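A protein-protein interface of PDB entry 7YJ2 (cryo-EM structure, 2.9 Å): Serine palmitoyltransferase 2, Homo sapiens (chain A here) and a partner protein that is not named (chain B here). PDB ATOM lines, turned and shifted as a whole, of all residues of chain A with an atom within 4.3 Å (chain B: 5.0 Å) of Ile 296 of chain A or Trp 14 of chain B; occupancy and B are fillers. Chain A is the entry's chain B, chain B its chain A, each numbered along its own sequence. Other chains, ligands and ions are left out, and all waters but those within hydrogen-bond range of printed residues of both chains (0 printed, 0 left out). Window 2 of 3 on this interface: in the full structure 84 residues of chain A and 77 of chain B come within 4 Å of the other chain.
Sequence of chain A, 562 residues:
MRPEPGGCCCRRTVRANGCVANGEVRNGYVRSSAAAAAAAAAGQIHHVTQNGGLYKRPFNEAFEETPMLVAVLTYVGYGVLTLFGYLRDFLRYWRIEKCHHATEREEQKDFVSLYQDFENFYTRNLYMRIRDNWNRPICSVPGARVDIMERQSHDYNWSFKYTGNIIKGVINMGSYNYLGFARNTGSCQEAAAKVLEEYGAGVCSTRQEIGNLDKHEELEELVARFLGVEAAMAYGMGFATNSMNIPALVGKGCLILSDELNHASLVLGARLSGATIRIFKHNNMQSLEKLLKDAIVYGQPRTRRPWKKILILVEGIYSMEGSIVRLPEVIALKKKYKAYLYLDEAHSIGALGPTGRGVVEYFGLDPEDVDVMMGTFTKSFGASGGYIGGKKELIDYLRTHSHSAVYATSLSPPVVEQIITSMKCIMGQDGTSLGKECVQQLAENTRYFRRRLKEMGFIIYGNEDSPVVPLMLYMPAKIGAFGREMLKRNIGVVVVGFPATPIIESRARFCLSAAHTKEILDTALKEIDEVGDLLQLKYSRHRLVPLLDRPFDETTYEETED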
ATOM      1  N   LEU A 292     -10.888 -23.429   5.613  1.00  0.00           N
ATOM      2  CA  LEU A 292     -10.358 -22.474   6.570  1.00  0.00           C
ATOM      3  C   LEU A 292     -11.439 -21.585   7.154  1.00  0.00           C
ATOM      4  O   LEU A 292     -11.303 -21.130   8.289  1.00  0.00           O
ATOM      5  CB  LEU A 292      -9.288 -21.626   5.888  1.00  0.00           C
ATOM      6  CG  LEU A 292      -8.303 -20.761   6.659  1.00  0.00           C
ATOM      7  CD1 LEU A 292      -7.528 -21.593   7.637  1.00  0.00           C
ATOM      8  CD2 LEU A 292      -7.358 -20.131   5.672  1.00  0.00           C
ATOM      9  N   LYS A 293     -12.507 -21.385   6.394  1.00  0.00           N
ATOM     10  CA  LYS A 293     -13.635 -20.574   6.816  1.00  0.00           C
ATOM     11  C   LYS A 293     -14.559 -21.389   7.706  1.00  0.00           C
ATOM     12  O   LYS A 293     -15.148 -20.869   8.637  1.00  0.00           O
ATOM     13  CB  LYS A 293     -14.395 -20.078   5.593  1.00  0.00           C
ATOM     14  CG  LYS A 293     -15.541 -19.139   5.907  1.00  0.00           C
ATOM     15  CD  LYS A 293     -16.508 -19.034   4.738  1.00  0.00           C
ATOM     16  CE  LYS A 293     -15.945 -19.695   3.492  1.00  0.00           C
ATOM     17  NZ  LYS A 293     -15.483 -18.693   2.495  1.00  0.00           N
ATOM     18  N   ASP A 294     -14.658 -22.678   7.417  1.00  0.00           N
ATOM     19  CA  ASP A 294     -15.514 -23.566   8.182  1.00  0.00           C
ATOM     20  C   ASP A 294     -14.902 -23.990   9.523  1.00  0.00           C
ATOM     21  O   ASP A 294     -15.531 -24.703  10.294  1.00  0.00           O
ATOM     22  CB  ASP A 294     -15.927 -24.760   7.319  1.00  0.00           C
ATOM     23  CG  ASP A 294     -15.648 -26.086   7.976  1.00  0.00           C
ATOM     24  OD1 ASP A 294     -14.475 -26.359   8.298  1.00  0.00           O
ATOM     25  OD2 ASP A 294     -16.604 -26.867   8.156  1.00  0.00           O
ATOM     26  N   ALA A 295     -13.677 -23.556   9.801  1.00  0.00           N
ATOM     27  CA  ALA A 295     -13.049 -23.870  11.069  1.00  0.00           C
ATOM     28  C   ALA A 295     -13.152 -22.735  12.067  1.00  0.00           C
ATOM     29  O   ALA A 295     -12.938 -22.960  13.257  1.00  0.00           O
ATOM     30  CB  ALA A 295     -11.578 -24.228  10.859  1.00  0.00           C
ATOM     31  N   ILE A 296     -13.469 -21.529  11.613  1.00  0.00           N
ATOM     32  CA  ILE A 296     -13.683 -20.395  12.500  1.00  0.00           C
ATOM     33  C   ILE A 296     -15.150 -20.190  12.824  1.00  0.00           C
ATOM     34  O   ILE A 296     -15.461 -19.437  13.757  1.00  0.00           O
ATOM     35  CB  ILE A 296     -13.070 -19.105  11.917  1.00  0.00           C
ATOM     36  CG1 ILE A 296     -11.601 -19.336  11.587  1.00  0.00           C
ATOM     37  CG2 ILE A 296     -13.137 -17.962  12.891  1.00  0.00           C
ATOM     38  CD1 ILE A 296     -10.953 -18.159  10.960  1.00  0.00           C
ATOM     39  N   VAL A 297     -16.063 -20.856  12.123  1.00  0.00           N
ATOM     40  CA  VAL A 297     -17.468 -20.758  12.484  1.00  0.00           C
ATOM     41  C   VAL A 297     -17.936 -21.914  13.356  1.00  0.00           C
ATOM     42  O   VAL A 297     -18.925 -21.753  14.085  1.00  0.00           O
ATOM     43  CB  VAL A 297     -18.378 -20.639  11.244  1.00  0.00           C
ATOM     44  CG1 VAL A 297     -18.009 -19.433  10.417  1.00  0.00           C
ATOM     45  CG2 VAL A 297     -18.341 -21.884  10.428  1.00  0.00           C
ATOM     46  N   TYR A 298     -17.255 -23.060  13.328  1.00  0.00           N
ATOM     47  CA  TYR A 298     -17.731 -24.241  14.034  1.00  0.00           C
ATOM     48  C   TYR A 298     -16.861 -24.678  15.198  1.00  0.00           C
ATOM     49  O   TYR A 298     -17.310 -25.503  15.990  1.00  0.00           O
ATOM     50  CB  TYR A 298     -17.874 -25.424  13.067  1.00  0.00           C
ATOM     51  CG  TYR A 298     -18.871 -25.173  11.971  1.00  0.00           C
ATOM     52  CD1 TYR A 298     -20.067 -24.541  12.237  1.00  0.00           C
ATOM     53  CD2 TYR A 298     -18.610 -25.552  10.668  1.00  0.00           C
ATOM     54  CE1 TYR A 298     -20.977 -24.295  11.242  1.00  0.00           C
ATOM     55  CE2 TYR A 298     -19.513 -25.310   9.662  1.00  0.00           C
ATOM     56  CZ  TYR A 298     -20.695 -24.682   9.953  1.00  0.00           C
ATOM     57  OH  TYR A 298     -21.608 -24.442   8.953  1.00  0.00           O
ATOM     58  N   PRO A 306     -13.627 -21.920  20.380  1.00  0.00           N
ATOM     59  CA  PRO A 306     -12.692 -21.388  19.386  1.00  0.00           C
ATOM     60  C   PRO A 306     -11.351 -22.103  19.435  1.00  0.00           C
ATOM     61  O   PRO A 306     -10.861 -22.464  20.504  1.00  0.00           O
ATOM     62  CB  PRO A 306     -12.555 -19.920  19.791  1.00  0.00           C
ATOM     63  CG  PRO A 306     -13.779 -19.625  20.515  1.00  0.00           C
ATOM     64  CD  PRO A 306     -14.135 -20.858  21.257  1.00  0.00           C
ATOM     65  N   TRP A 307     -10.757 -22.308  18.265  1.00  0.00           N
ATOM     66  CA  TRP A 307      -9.426 -22.892  18.205  1.00  0.00           C
ATOM     67  C   TRP A 307      -8.425 -21.932  18.820  1.00  0.00           C
ATOM     68  O   TRP A 307      -8.558 -20.716  18.688  1.00  0.00           O
ATOM     69  CB  TRP A 307      -9.027 -23.181  16.762  1.00  0.00           C
ATOM     70  CG  TRP A 307      -9.850 -24.182  16.045  1.00  0.00           C
ATOM     71  CD1 TRP A 307     -10.791 -23.932  15.117  1.00  0.00           C
ATOM     72  CD2 TRP A 307      -9.785 -25.597  16.175  1.00  0.00           C
ATOM     73  NE1 TRP A 307     -11.324 -25.093  14.654  1.00  0.00           N
ATOM     74  CE2 TRP A 307     -10.723 -26.135  15.296  1.00  0.00           C
ATOM     75  CE3 TRP A 307      -9.020 -26.462  16.948  1.00  0.00           C
ATOM     76  CZ2 TRP A 307     -10.918 -27.493  15.167  1.00  0.00           C
ATOM     77  CZ3 TRP A 307      -9.218 -27.804  16.818  1.00  0.00           C
ATOM     78  CH2 TRP A 307     -10.156 -28.309  15.939  1.00  0.00           C
ATOM     79  N   ILE A 310      -4.337 -21.602  14.313  1.00  0.00           N
ATOM     80  CA  ILE A 310      -4.382 -22.397  13.090  1.00  0.00           C
ATOM     81  C   ILE A 310      -3.047 -22.260  12.377  1.00  0.00           C
ATOM     82  O   ILE A 310      -2.559 -21.146  12.187  1.00  0.00           O
ATOM     83  CB  ILE A 310      -5.534 -21.959  12.166  1.00  0.00           C
ATOM     84  CG1 ILE A 310      -6.880 -22.193  12.843  1.00  0.00           C
ATOM     85  CG2 ILE A 310      -5.483 -22.704  10.855  1.00  0.00           C
ATOM     86  CD1 ILE A 310      -8.033 -21.628  12.108  1.00  0.00           C
ATOM     87  N   TYR A 337      -7.684 -14.450   7.190  1.00  0.00           N
ATOM     88  CA  TYR A 337      -8.232 -15.361   8.181  1.00  0.00           C
ATOM     89  C   TYR A 337      -7.331 -15.504   9.396  1.00  0.00           C
ATOM     90  O   TYR A 337      -7.628 -16.309  10.274  1.00  0.00           O
ATOM     91  CB  TYR A 337      -8.489 -16.729   7.552  1.00  0.00           C
ATOM     92  CG  TYR A 337      -9.628 -16.716   6.572  1.00  0.00           C
ATOM     93  CD1 TYR A 337     -10.913 -16.470   6.989  1.00  0.00           C
ATOM     94  CD2 TYR A 337      -9.412 -16.918   5.226  1.00  0.00           C
ATOM     95  CE1 TYR A 337     -11.950 -16.445   6.104  1.00  0.00           C
ATOM     96  CE2 TYR A 337     -10.443 -16.890   4.334  1.00  0.00           C
ATOM     97  CZ  TYR A 337     -11.712 -16.657   4.780  1.00  0.00           C
ATOM     98  OH  TYR A 337     -12.756 -16.630   3.896  1.00  0.00           O
ATOM     99  N   LYS A 338      -6.294 -14.687   9.484  1.00  0.00           N
ATOM    100  CA  LYS A 338      -5.403 -14.673  10.642  1.00  0.00           C
ATOM    101  C   LYS A 338      -4.758 -15.990  11.058  1.00  0.00           C
ATOM    102  O   LYS A 338      -4.670 -16.297  12.242  1.00  0.00           O
ATOM    103  CB  LYS A 338      -6.124 -14.064  11.842  1.00  0.00           C
ATOM    104  CG  LYS A 338      -6.205 -12.550  11.812  1.00  0.00           C
ATOM    105  CD  LYS A 338      -7.493 -12.061  12.444  1.00  0.00           C
ATOM    106  CE  LYS A 338      -8.708 -12.683  11.782  1.00  0.00           C
ATOM    107  NZ  LYS A 338      -9.969 -12.103  12.315  1.00  0.00           N
ATOM    108  N   LEU B  10     -18.739 -13.690  12.884  1.00  0.00           N
ATOM    109  CA  LEU B  10     -17.975 -14.736  13.551  1.00  0.00           C
ATOM    110  C   LEU B  10     -16.541 -14.765  13.054  1.00  0.00           C
ATOM    111  O   LEU B  10     -15.601 -14.806  13.852  1.00  0.00           O
ATOM    112  CB  LEU B  10     -18.636 -16.089  13.314  1.00  0.00           C
ATOM    113  CG  LEU B  10     -19.705 -16.557  14.287  1.00  0.00           C
ATOM    114  CD1 LEU B  10     -20.960 -15.761  14.095  1.00  0.00           C
ATOM    115  CD2 LEU B  10     -19.993 -18.014  14.047  1.00  0.00           C
ATOM    116  N   ILE B  11     -16.354 -14.732  11.735  1.00  0.00           N
ATOM    117  CA  ILE B  11     -15.012 -14.746  11.166  1.00  0.00           C
ATOM    118  C   ILE B  11     -14.213 -13.515  11.543  1.00  0.00           C
ATOM    119  O   ILE B  11     -12.982 -13.578  11.583  1.00  0.00           O
ATOM    120  CB  ILE B  11     -15.107 -14.910   9.637  1.00  0.00           C
ATOM    121  CG1 ILE B  11     -15.731 -16.259   9.293  1.00  0.00           C
ATOM    122  CG2 ILE B  11     -13.758 -14.804   8.983  1.00  0.00           C
ATOM    123  CD1 ILE B  11     -16.091 -16.416   7.850  1.00  0.00           C
ATOM    124  N   GLU B  12     -14.909 -12.418  11.805  1.00  0.00           N
ATOM    125  CA  GLU B  12     -14.277 -11.143  12.112  1.00  0.00           C
ATOM    126  C   GLU B  12     -13.893 -10.914  13.563  1.00  0.00           C
ATOM    127  O   GLU B  12     -12.943 -10.194  13.845  1.00  0.00           O
ATOM    128  CB  GLU B  12     -15.181 -10.004  11.645  1.00  0.00           C
ATOM    129  CG  GLU B  12     -14.725  -9.346  10.359  1.00  0.00           C
ATOM    130  CD  GLU B  12     -14.039  -8.026  10.616  1.00  0.00           C
ATOM    131  OE1 GLU B  12     -14.039  -7.587  11.784  1.00  0.00           O
ATOM    132  OE2 GLU B  12     -13.503  -7.434   9.657  1.00  0.00           O
ATOM    133  N   GLU B  13     -14.634 -11.506  14.487  1.00  0.00           N
ATOM    134  CA  GLU B  13     -14.334 -11.322  15.901  1.00  0.00           C
ATOM    135  C   GLU B  13     -13.285 -12.282  16.439  1.00  0.00           C
ATOM    136  O   GLU B  13     -12.828 -12.086  17.566  1.00  0.00           O
ATOM    137  CB  GLU B  13     -15.585 -11.489  16.765  1.00  0.00           C
ATOM    138  CG  GLU B  13     -16.152 -12.885  16.757  1.00  0.00           C
ATOM    139  CD  GLU B  13     -17.417 -13.008  17.575  1.00  0.00           C
ATOM    140  OE1 GLU B  13     -17.862 -11.988  18.133  1.00  0.00           O
ATOM    141  OE2 GLU B  13     -17.962 -14.125  17.672  1.00  0.00           O
ATOM    142  N   TRP B  14     -12.910 -13.315  15.681  1.00  0.00           N
ATOM    143  CA  TRP B  14     -11.978 -14.321  16.173  1.00  0.00           C
ATOM    144  C   TRP B  14     -10.604 -13.721  16.414  1.00  0.00           C
ATOM    145  O   TRP B  14     -10.191 -12.783  15.736  1.00  0.00           O
ATOM    146  CB  TRP B  14     -11.859 -15.478  15.186  1.00  0.00           C
ATOM    147  CG  TRP B  14     -11.040 -16.632  15.723  1.00  0.00           C
ATOM    148  CD1 TRP B  14     -11.263 -17.332  16.869  1.00  0.00           C
ATOM    149  CD2 TRP B  14      -9.866 -17.203  15.133  1.00  0.00           C
ATOM    150  NE1 TRP B  14     -10.305 -18.293  17.032  1.00  0.00           N
ATOM    151  CE2 TRP B  14      -9.437 -18.237  15.977  1.00  0.00           C
ATOM    152  CE3 TRP B  14      -9.136 -16.935  13.977  1.00  0.00           C
ATOM    153  CZ2 TRP B  14      -8.322 -18.999  15.700  1.00  0.00           C
ATOM    154  CZ3 TRP B  14      -8.038 -17.692  13.711  1.00  0.00           C
ATOM    155  CH2 TRP B  14      -7.638 -18.712  14.566  1.00  0.00           C
ATOM    156  N   GLN B  15      -9.898 -14.265  17.392  1.00  0.00           N
ATOM    157  CA  GLN B  15      -8.589 -13.738  17.737  1.00  0.00           C
ATOM    158  C   GLN B  15      -7.655 -14.851  18.192  1.00  0.00           C
ATOM    159  O   GLN B  15      -7.821 -15.387  19.292  1.00  0.00           O
ATOM    160  CB  GLN B  15      -8.726 -12.684  18.832  1.00  0.00           C
ATOM    161  CG  GLN B  15      -7.682 -11.596  18.781  1.00  0.00           C
ATOM    162  CD  GLN B  15      -7.556 -10.975  17.411  1.00  0.00           C
ATOM    163  OE1 GLN B  15      -8.555 -10.670  16.761  1.00  0.00           O
ATOM    164  NE2 GLN B  15      -6.322 -10.777  16.963  1.00  0.00           N
ATOM    165  N   PRO B  16      -6.656 -15.208  17.399  1.00  0.00           N
ATOM    166  CA  PRO B  16      -5.740 -16.281  17.787  1.00  0.00           C
ATOM    167  C   PRO B  16      -4.755 -15.842  18.862  1.00  0.00           C
ATOM    168  O   PRO B  16      -4.575 -14.661  19.145  1.00  0.00           O
ATOM    169  CB  PRO B  16      -5.016 -16.593  16.484  1.00  0.00           C
ATOM    170  CG  PRO B  16      -5.053 -15.345  15.739  1.00  0.00           C
ATOM    171  CD  PRO B  16      -6.335 -14.672  16.070  1.00  0.00           C
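Printed residues of chain B that touch a printed residue of chain A: Leu 10, Ile 11, Glu 12, Trp 14 and Pro 16.
Hydrophobic or aromatic side chains of chain B within 4 Å of the printed part of chain A: Leu 10, Ile 11, Trp 14 and Pro 16.
Of the 12 printed residues of chain A, 8 touch a printed residue of chain B.
Hydrophobic or aromatic side chains of chain A within 4 Å of the printed part of chain B: Ile 296, Pro 306, Ile 310 and Tyr 337.
Among the printed residues, 12 pairs touch across the chains.
The indole nitrogen (NE1) of Trp 307 of chain A sits close to the backbone carbonyl oxygen (O) of Ala 295 of chain A (3.0 Å).
Of chain B, only Trp 14 (3.6 Å) comes within 4 Å of Ile 296 of chain A.
Trp 14 of chain B touches six residues of chain A.
Of the printed residues of chain B, Ile 310 of chain A touches Trp 14.
Of the printed residues of chain A, Pro 16 of chain B touches Lys 338 (3.6 Å).
Of the printed residues of chain B, Lys 338 of chain A touches Ile 11, Glu 12, Trp 14 and Pro 16.
Printed residues of chain B within 4 Å of Pro 306 of chain A: Trp 14 (3.9 Å).
Tyr 298 of chain A touches none of the printed residues of chain B.
Leu 292 of chain A touches none of the printed residues of chain B.
The nearest printed residue of chain B that does not touch Ile 296 of chain A is Ile 11 of chain B (4.1 Å).
The nearest printed residue of chain B that does not touch Ile 310 of chain A is Pro 16 of chain B (5.5 Å).
Among the printed residues, merely in contact across the chains: Lys 293 of chain A with Ile 11 of chain B, Ile 296 of chain A with Trp 14 of chain B, Lys 338 of chain A with Pro 16 of chain B, Tyr 337 of chain A with Trp 14 of chain B, Tyr 337 of chain A with Ile 11 of chain B, Ile 310 of chain A with Trp 14 of chain B, Lys 338 of chain A with Glu 12 of chain B, Val 297 of chain A with Leu 10 of chain B and Pro 306 of chain A with Trp 14 of chain B.
NE1 of Trp 14 of chain B sits at hydrogen-bond distance from O of Trp 307 of chain A, at 3.4 Å.
The side-chain amino group of Lys 338 of chain A is in hydrogen-bond range of the backbone carbonyl oxygen of Ile 11 of chain B (3.4 Å).
NZ of Lys 338 of chain A lies within hydrogen-bond range of O of Trp 14 of chain B (3.5 Å).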
